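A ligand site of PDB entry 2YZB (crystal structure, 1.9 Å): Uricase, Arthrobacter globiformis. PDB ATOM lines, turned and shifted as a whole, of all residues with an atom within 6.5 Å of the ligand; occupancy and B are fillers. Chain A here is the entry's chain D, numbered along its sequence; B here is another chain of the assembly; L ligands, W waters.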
ATOM      1  N   SER A 161       2.126   8.106  13.936  1.00  0.00           N
ATOM      2  CA  SER A 161       1.322   6.923  13.646  1.00  0.00           C
ATOM      3  C   SER A 161       1.186   6.746  12.141  1.00  0.00           C
ATOM      4  O   SER A 161       0.895   7.695  11.406  1.00  0.00           O
ATOM      5  CB  SER A 161      -0.068   7.052  14.284  1.00  0.00           C
ATOM      6  OG  SER A 161      -0.890   5.955  13.910  1.00  0.00           O
ATOM      7  N   GLU A 162       1.395   5.523  11.688  1.00  0.00           N
ATOM      8  CA  GLU A 162       1.290   5.189  10.269  1.00  0.00           C
ATOM      9  C   GLU A 162       0.475   3.919  10.104  1.00  0.00           C
ATOM     10  O   GLU A 162       0.266   3.161  11.051  1.00  0.00           O
ATOM     11  CB  GLU A 162       2.681   4.916   9.670  1.00  0.00           C
ATOM     12  CG  GLU A 162       3.734   5.998   9.864  1.00  0.00           C
ATOM     13  CD  GLU A 162       5.070   5.614   9.258  1.00  0.00           C
ATOM     14  OE1 GLU A 162       5.085   5.033   8.149  1.00  0.00           O
ATOM     15  OE2 GLU A 162       6.115   5.903   9.864  1.00  0.00           O
ATOM     16  N   PHE A 163       0.015   3.697   8.878  1.00  0.00           N
ATOM     17  CA  PHE A 163      -0.696   2.477   8.548  1.00  0.00           C
ATOM     18  C   PHE A 163      -0.613   2.272   7.050  1.00  0.00           C
ATOM     19  O   PHE A 163      -1.308   2.919   6.266  1.00  0.00           O
ATOM     20  CB  PHE A 163      -2.152   2.499   8.989  1.00  0.00           C
ATOM     21  CG  PHE A 163      -2.806   1.149   8.939  1.00  0.00           C
ATOM     22  CD1 PHE A 163      -2.302   0.102   9.707  1.00  0.00           C
ATOM     23  CD2 PHE A 163      -3.856   0.892   8.072  1.00  0.00           C
ATOM     24  CE1 PHE A 163      -2.844  -1.183   9.615  1.00  0.00           C
ATOM     25  CE2 PHE A 163      -4.410  -0.392   7.973  1.00  0.00           C
ATOM     26  CZ  PHE A 163      -3.895  -1.426   8.750  1.00  0.00           C
ATOM     27  N   LEU A 174      -9.273   1.915   1.493  1.00  0.00           N
ATOM     28  CA  LEU A 174      -8.420   2.691   2.402  1.00  0.00           C
ATOM     29  C   LEU A 174      -7.108   3.087   1.732  1.00  0.00           C
ATOM     30  O   LEU A 174      -6.500   2.295   1.008  1.00  0.00           O
ATOM     31  CB  LEU A 174      -8.118   1.879   3.667  1.00  0.00           C
ATOM     32  CG  LEU A 174      -7.281   2.530   4.783  1.00  0.00           C
ATOM     33  CD1 LEU A 174      -7.983   3.792   5.293  1.00  0.00           C
ATOM     34  CD2 LEU A 174      -7.084   1.534   5.906  1.00  0.00           C
ATOM     35  N   ARG A 180      -1.013   9.990  10.599  1.00  0.00           N
ATOM     36  CA  ARG A 180      -2.424  10.045  10.956  1.00  0.00           C
ATOM     37  C   ARG A 180      -2.555  10.209  12.467  1.00  0.00           C
ATOM     38  O   ARG A 180      -1.576  10.060  13.197  1.00  0.00           O
ATOM     39  CB  ARG A 180      -3.137   8.746  10.550  1.00  0.00           C
ATOM     40  CG  ARG A 180      -2.672   7.526  11.341  1.00  0.00           C
ATOM     41  CD  ARG A 180      -3.463   6.272  11.008  1.00  0.00           C
ATOM     42  NE  ARG A 180      -3.099   5.142  11.857  1.00  0.00           N
ATOM     43  CZ  ARG A 180      -3.715   3.958  11.863  1.00  0.00           C
ATOM     44  NH1 ARG A 180      -4.743   3.741  11.062  1.00  0.00           N
ATOM     45  NH2 ARG A 180      -3.301   2.995  12.682  1.00  0.00           N
ATOM     46  N   LEU A 182      -3.766   8.893  16.035  1.00  0.00           N
ATOM     47  CA  LEU A 182      -3.999   7.588  16.645  1.00  0.00           C
ATOM     48  C   LEU A 182      -4.636   7.900  17.999  1.00  0.00           C
ATOM     49  O   LEU A 182      -3.969   8.444  18.874  1.00  0.00           O
ATOM     50  CB  LEU A 182      -2.696   6.815  16.848  1.00  0.00           C
ATOM     51  CG  LEU A 182      -2.881   5.446  17.515  1.00  0.00           C
ATOM     52  CD1 LEU A 182      -3.783   4.566  16.649  1.00  0.00           C
ATOM     53  CD2 LEU A 182      -1.546   4.780  17.735  1.00  0.00           C
ATOM     54  N   SER A 219       4.059   4.280  16.007  1.00  0.00           N
ATOM     55  CA  SER A 219       3.124   3.256  15.578  1.00  0.00           C
ATOM     56  C   SER A 219       2.994   2.975  14.087  1.00  0.00           C
ATOM     57  O   SER A 219       2.773   3.886  13.279  1.00  0.00           O
ATOM     58  CB  SER A 219       1.730   3.571  16.138  1.00  0.00           C
ATOM     59  OG  SER A 219       0.839   2.498  15.882  1.00  0.00           O
ATOM     60  N   LEU A 220       3.103   1.700  13.732  1.00  0.00           N
ATOM     61  CA  LEU A 220       2.956   1.254  12.359  1.00  0.00           C
ATOM     62  C   LEU A 220       1.625   0.515  12.265  1.00  0.00           C
ATOM     63  O   LEU A 220       1.210   0.083  11.189  1.00  0.00           O
ATOM     64  CB  LEU A 220       4.114   0.322  11.967  1.00  0.00           C
ATOM     65  CG  LEU A 220       5.513   0.972  12.020  1.00  0.00           C
ATOM     66  CD1 LEU A 220       6.576  -0.028  11.609  1.00  0.00           C
ATOM     67  CD2 LEU A 220       5.549   2.185  11.113  1.00  0.00           C
ATOM     68  N   ALA A 221       0.953   0.392  13.414  1.00  0.00           N
ATOM     69  CA  ALA A 221      -0.350  -0.258  13.527  1.00  0.00           C
ATOM     70  C   ALA A 221      -0.792  -0.195  14.988  1.00  0.00           C
ATOM     71  O   ALA A 221       0.046  -0.118  15.888  1.00  0.00           O
ATOM     72  CB  ALA A 221      -0.277  -1.712  13.067  1.00  0.00           C
ATOM     73  N   LEU A 222      -2.109  -0.242  15.224  1.00  0.00           N
ATOM     74  CA  LEU A 222      -2.614  -0.196  16.591  1.00  0.00           C
ATOM     75  C   LEU A 222      -2.183  -1.494  17.277  1.00  0.00           C
ATOM     76  O   LEU A 222      -1.909  -1.503  18.470  1.00  0.00           O
ATOM     77  CB  LEU A 222      -4.146  -0.085  16.619  1.00  0.00           C
ATOM     78  CG  LEU A 222      -4.746   0.741  17.769  1.00  0.00           C
ATOM     79  CD1 LEU A 222      -6.228   0.390  17.943  1.00  0.00           C
ATOM     80  CD2 LEU A 222      -4.011   0.491  19.051  1.00  0.00           C
ATOM     81  N   GLN A 223      -2.126  -2.571  16.511  1.00  0.00           N
ATOM     82  CA  GLN A 223      -1.715  -3.864  17.038  1.00  0.00           C
ATOM     83  C   GLN A 223      -0.287  -3.785  17.607  1.00  0.00           C
ATOM     84  O   GLN A 223       0.006  -4.338  18.669  1.00  0.00           O
ATOM     85  CB  GLN A 223      -1.769  -4.934  15.937  1.00  0.00           C
ATOM     86  CG  GLN A 223      -3.189  -5.290  15.509  1.00  0.00           C
ATOM     87  CD  GLN A 223      -3.719  -4.432  14.375  1.00  0.00           C
ATOM     88  OE1 GLN A 223      -3.457  -3.221  14.314  1.00  0.00           O
ATOM     89  NE2 GLN A 223      -4.485  -5.046  13.489  1.00  0.00           N
ATOM     90  N   ASN A 249     -10.089   2.006  17.876  1.00  0.00           N
ATOM     91  CA  ASN A 249      -9.361   2.983  17.090  1.00  0.00           C
ATOM     92  C   ASN A 249     -10.377   4.079  16.809  1.00  0.00           C
ATOM     93  O   ASN A 249     -11.198   3.946  15.906  1.00  0.00           O
ATOM     94  CB  ASN A 249      -8.852   2.365  15.786  1.00  0.00           C
ATOM     95  CG  ASN A 249      -7.714   3.159  15.156  1.00  0.00           C
ATOM     96  OD1 ASN A 249      -7.631   4.375  15.312  1.00  0.00           O
ATOM     97  ND2 ASN A 249      -6.837   2.481  14.427  1.00  0.00           N
ATOM     98  N   HIS A 251     -11.634   6.885  15.178  1.00  0.00           N
ATOM     99  CA  HIS A 251     -11.318   7.592  13.953  1.00  0.00           C
ATOM    100  C   HIS A 251     -11.463   9.099  13.959  1.00  0.00           C
ATOM    101  O   HIS A 251     -12.485   9.651  14.354  1.00  0.00           O
ATOM    102  CB  HIS A 251     -12.131   6.998  12.806  1.00  0.00           C
ATOM    103  CG  HIS A 251     -11.779   5.574  12.501  1.00  0.00           C
ATOM    104  ND1 HIS A 251     -12.719   4.565  12.475  1.00  0.00           N
ATOM    105  CD2 HIS A 251     -10.577   4.986  12.264  1.00  0.00           C
ATOM    106  CE1 HIS A 251     -12.110   3.412  12.251  1.00  0.00           C
ATOM    107  NE2 HIS A 251     -10.815   3.639  12.124  1.00  0.00           N
ATOM    108  N   GLY A 277     -12.454   0.949  14.973  1.00  0.00           N
ATOM    109  CA  GLY A 277     -11.665  -0.259  14.936  1.00  0.00           C
ATOM    110  C   GLY A 277     -11.607  -0.778  16.354  1.00  0.00           C
ATOM    111  O   GLY A 277     -11.719   0.004  17.304  1.00  0.00           O
ATOM    112  N   ILE A 279      -9.147  -3.389  18.378  1.00  0.00           N
ATOM    113  CA  ILE A 279      -7.954  -4.238  18.391  1.00  0.00           C
ATOM    114  C   ILE A 279      -7.781  -4.804  19.802  1.00  0.00           C
ATOM    115  O   ILE A 279      -7.672  -4.045  20.773  1.00  0.00           O
ATOM    116  CB  ILE A 279      -6.711  -3.409  17.974  1.00  0.00           C
ATOM    117  CG1 ILE A 279      -6.680  -3.219  16.452  1.00  0.00           C
ATOM    118  CG2 ILE A 279      -5.435  -4.096  18.412  1.00  0.00           C
ATOM    119  CD1 ILE A 279      -7.906  -2.516  15.859  1.00  0.00           C
ATOM    120  N   TYR B  20      -9.099  -8.652  15.943  1.00  0.00           N
ATOM    121  CA  TYR B  20      -9.259  -7.250  15.595  1.00  0.00           C
ATOM    122  C   TYR B  20     -10.247  -7.107  14.443  1.00  0.00           C
ATOM    123  O   TYR B  20     -10.440  -8.034  13.657  1.00  0.00           O
ATOM    124  CB  TYR B  20      -7.914  -6.655  15.159  1.00  0.00           C
ATOM    125  CG  TYR B  20      -7.598  -6.961  13.716  1.00  0.00           C
ATOM    126  CD1 TYR B  20      -7.266  -8.248  13.316  1.00  0.00           C
ATOM    127  CD2 TYR B  20      -7.735  -5.978  12.737  1.00  0.00           C
ATOM    128  CE1 TYR B  20      -7.082  -8.566  11.972  1.00  0.00           C
ATOM    129  CE2 TYR B  20      -7.560  -6.276  11.394  1.00  0.00           C
ATOM    130  CZ  TYR B  20      -7.234  -7.576  11.021  1.00  0.00           C
ATOM    131  OH  TYR B  20      -7.093  -7.877   9.683  1.00  0.00           O
ATOM    132  N   GLY B  21     -10.867  -5.943  14.354  1.00  0.00           N
ATOM    133  CA  GLY B  21     -11.797  -5.727  13.260  1.00  0.00           C
ATOM    134  C   GLY B  21     -12.507  -4.404  13.422  1.00  0.00           C
ATOM    135  O   GLY B  21     -12.040  -3.527  14.158  1.00  0.00           O
ATOM    136  N   LYS B  22     -13.631  -4.268  12.738  1.00  0.00           N
ATOM    137  CA  LYS B  22     -14.408  -3.041  12.843  1.00  0.00           C
ATOM    138  C   LYS B  22     -15.613  -3.315  13.723  1.00  0.00           C
ATOM    139  O   LYS B  22     -16.358  -4.277  13.511  1.00  0.00           O
ATOM    140  CB  LYS B  22     -14.876  -2.577  11.472  1.00  0.00           C
ATOM    141  CG  LYS B  22     -15.568  -1.231  11.510  1.00  0.00           C
ATOM    142  CD  LYS B  22     -14.564  -0.106  11.722  1.00  0.00           C
ATOM    143  CE  LYS B  22     -13.729   0.103  10.481  1.00  0.00           C
ATOM    144  NZ  LYS B  22     -12.809   1.265  10.610  1.00  0.00           N
ATOM    145  N   ASN B  61       2.195  -5.272   8.323  1.00  0.00           N
ATOM    146  CA  ASN B  61       0.770  -5.393   8.035  1.00  0.00           C
ATOM    147  C   ASN B  61       0.330  -6.248   6.855  1.00  0.00           C
ATOM    148  O   ASN B  61      -0.841  -6.186   6.454  1.00  0.00           O
ATOM    149  CB  ASN B  61       0.162  -3.994   7.886  1.00  0.00           C
ATOM    150  CG  ASN B  61       0.232  -3.183   9.159  1.00  0.00           C
ATOM    151  OD1 ASN B  61      -0.091  -3.685  10.239  1.00  0.00           O
ATOM    152  ND2 ASN B  61       0.647  -1.923   9.051  1.00  0.00           N
ATOM    153  N   VAL B  64      -2.708  -7.978   7.704  1.00  0.00           N
ATOM    154  CA  VAL B  64      -3.781  -7.171   8.264  1.00  0.00           C
ATOM    155  C   VAL B  64      -4.837  -6.641   7.298  1.00  0.00           C
ATOM    156  O   VAL B  64      -4.668  -5.579   6.695  1.00  0.00           O
ATOM    157  CB  VAL B  64      -3.206  -5.982   9.079  1.00  0.00           C
ATOM    158  CG1 VAL B  64      -4.329  -5.229   9.763  1.00  0.00           C
ATOM    159  CG2 VAL B  64      -2.219  -6.501  10.115  1.00  0.00           C
ATOM    160  N   VAL B  65      -5.914  -7.403   7.161  1.00  0.00           N
ATOM    161  CA  VAL B  65      -7.050  -7.006   6.343  1.00  0.00           C
ATOM    162  C   VAL B  65      -7.593  -5.799   7.110  1.00  0.00           C
ATOM    163  O   VAL B  65      -8.122  -5.954   8.213  1.00  0.00           O
ATOM    164  CB  VAL B  65      -8.136  -8.088   6.304  1.00  0.00           C
ATOM    165  CG1 VAL B  65      -9.369  -7.563   5.612  1.00  0.00           C
ATOM    166  CG2 VAL B  65      -7.613  -9.327   5.589  1.00  0.00           C
ATOM    167  N   ALA B  66      -7.438  -4.614   6.537  1.00  0.00           N
ATOM    168  CA  ALA B  66      -7.877  -3.376   7.169  1.00  0.00           C
ATOM    169  C   ALA B  66      -9.269  -3.419   7.804  1.00  0.00           C
ATOM    170  O   ALA B  66     -10.198  -4.029   7.271  1.00  0.00           O
ATOM    171  CB  ALA B  66      -7.813  -2.241   6.146  1.00  0.00           C
ATOM    172  N   THR B  67      -9.418  -2.784   8.957  1.00  0.00           N
ATOM    173  CA  THR B  67     -10.720  -2.765   9.606  1.00  0.00           C
ATOM    174  C   THR B  67     -11.655  -1.995   8.676  1.00  0.00           C
ATOM    175  O   THR B  67     -12.851  -2.268   8.615  1.00  0.00           O
ATOM    176  CB  THR B  67     -10.681  -2.073  11.010  1.00  0.00           C
ATOM    177  OG1 THR B  67     -10.292  -0.708  10.865  1.00  0.00           O
ATOM    178  CG2 THR B  67      -9.692  -2.789  11.946  1.00  0.00           C
ATOM    179  N   ASP B  68     -11.102  -1.036   7.920  1.00  0.00           N
ATOM    180  CA  ASP B  68     -11.898  -0.261   6.983  1.00  0.00           C
ATOM    181  C   ASP B  68     -12.429  -1.166   5.884  1.00  0.00           C
ATOM    182  O   ASP B  68     -13.526  -0.965   5.378  1.00  0.00           O
ATOM    183  CB  ASP B  68     -11.067   0.857   6.341  1.00  0.00           C
ATOM    184  CG  ASP B  68     -11.885   1.719   5.388  1.00  0.00           C
ATOM    185  OD1 ASP B  68     -12.631   2.602   5.862  1.00  0.00           O
ATOM    186  OD2 ASP B  68     -11.808   1.501   4.160  1.00  0.00           O
ATOM    187  N   THR B  69     -11.640  -2.173   5.521  1.00  0.00           N
ATOM    188  CA  THR B  69     -12.037  -3.115   4.484  1.00  0.00           C
ATOM    189  C   THR B  69     -13.150  -3.998   5.017  1.00  0.00           C
ATOM    190  O   THR B  69     -14.094  -4.323   4.295  1.00  0.00           O
ATOM    191  CB  THR B  69     -10.865  -4.002   4.051  1.00  0.00           C
ATOM    192  OG1 THR B  69      -9.839  -3.190   3.469  1.00  0.00           O
ATOM    193  CG2 THR B  69     -11.328  -5.031   3.030  1.00  0.00           C
ATOM    194  N   GLN B  70     -13.033  -4.406   6.282  1.00  0.00           N
ATOM    195  CA  GLN B  70     -14.053  -5.250   6.884  1.00  0.00           C
ATOM    196  C   GLN B  70     -15.361  -4.464   6.888  1.00  0.00           C
ATOM    197  O   GLN B  70     -16.424  -5.017   6.596  1.00  0.00           O
ATOM    198  CB  GLN B  70     -13.651  -5.636   8.305  1.00  0.00           C
ATOM    199  CG  GLN B  70     -12.456  -6.589   8.343  1.00  0.00           C
ATOM    200  CD  GLN B  70     -12.076  -7.016   9.744  1.00  0.00           C
ATOM    201  OE1 GLN B  70     -12.906  -7.501  10.513  1.00  0.00           O
ATOM    202  NE2 GLN B  70     -10.799  -6.865  10.087  1.00  0.00           N
HETATM  203  N1  LIG L   1      -4.985  -1.487  12.481  1.00  0.00           N
HETATM  204  C1  LIG L   1      -4.602  -0.146  12.512  1.00  0.00           C
HETATM  205  C2  LIG L   1      -6.001  -2.019  11.676  1.00  0.00           C
HETATM  206  N2  LIG L   1      -5.277   0.757  11.714  1.00  0.00           N
HETATM  207  O1  LIG L   1      -3.718   0.248  13.229  1.00  0.00           O
HETATM  208  C3  LIG L   1      -6.257   0.348  10.921  1.00  0.00           C
HETATM  209  C4  LIG L   1      -6.662  -0.982  10.857  1.00  0.00           C
HETATM  210  N3  LIG L   1      -6.984   1.107  10.098  1.00  0.00           N
HETATM  211  O2  LIG L   1      -6.254  -3.226  11.719  1.00  0.00           O
HETATM  212  N4  LIG L   1      -7.655  -1.060   9.978  1.00  0.00           N
HETATM  213  C5  LIG L   1      -7.813   0.221   9.547  1.00  0.00           C
HETATM  214  O3  LIG L   1      -8.642   0.531   8.735  1.00  0.00           O
HETATM  215  O   HOH W   1      -8.169   3.953   9.090  1.00  0.00           O
HETATM  216  O   HOH W   2      -9.046   0.455  13.012  1.00  0.00           O
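Phe 163 touches the ligand. CD2 of Leu 174 touches O3 of the ligand, at 3.4 Å. CA of Ala 221 touches O1 of the ligand, 3.4 Å away. ND2 of Asn 249 touches N2 of the ligand, at 3.6 Å. Tyr 20 of chain B touches the ligand (CD2 to O2, 3.3 Å). CG1 of Val 64 of chain B touches O2 of the ligand, at 3.4 Å. C of Ala 66 of chain B touches N4 of the ligand, 3.6 Å away. Hydrophobic or aromatic side chains within 4 Å of the ligand: Phe 163, Leu 174, Ala 221, Leu 222, Tyr 20 of chain B, Val 64 of chain B and Ala 66 of chain B. Within 4 Å of the ligand: Phe 163, Leu 174, Arg 180, Ala 221, Leu 222, Gln 223, Asn 249, Tyr 20 of chain B, Val 64 of chain B, Ala 66 of chain B, Thr 67 of chain B and Asp 68 of chain B. The nearest printed residue that does not touch the ligand is Ile 279 (4.5 Å).
O of Ala 221 sits at hydrogen-bond distance from OG of Ser 219, 2.7 Å away. N of Asn 249 is in hydrogen-bond range of O of Gly 277 (2.6 Å). The backbone NH (N) of Arg 180 sits at hydrogen-bond distance from the backbone carbonyl oxygen (O) of Ser 161, 3.1 Å away. O of Val 65 of chain B sits at hydrogen-bond distance from OH of Tyr 20 of chain B (2.6 Å). The side-chain hydroxyl (OG1) of Thr 67 of chain B lies within hydrogen-bond range of the side-chain amino group (NZ) of Lys 22 of chain B (3.2 Å).
The backbone NH (N) of Thr 67 of chain B sits at hydrogen-bond distance from an oxygen (O3) of the ligand. O1 of the ligand is in hydrogen-bond range of NH2 of Arg 180, at 2.8 Å. N of Leu 222 is in hydrogen-bond range of O1 of the ligand (2.6 Å). The side-chain hydroxyl (OG1) of Thr 67 of chain B is in hydrogen-bond range of a nitrogen (N4) of the ligand, at 2.8 Å. The side-chain amide oxygen of Gln 223 lies within hydrogen-bond range of a nitrogen (N1) of the ligand (2.9 Å). N of Asp 68 of chain B lies within hydrogen-bond range of O3 of the ligand.
Water W2 lies within hydrogen-bond range of OG1 of Thr 67 of chain B (2.7 Å) and ND2 of Asn 249 (3.3 Å).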
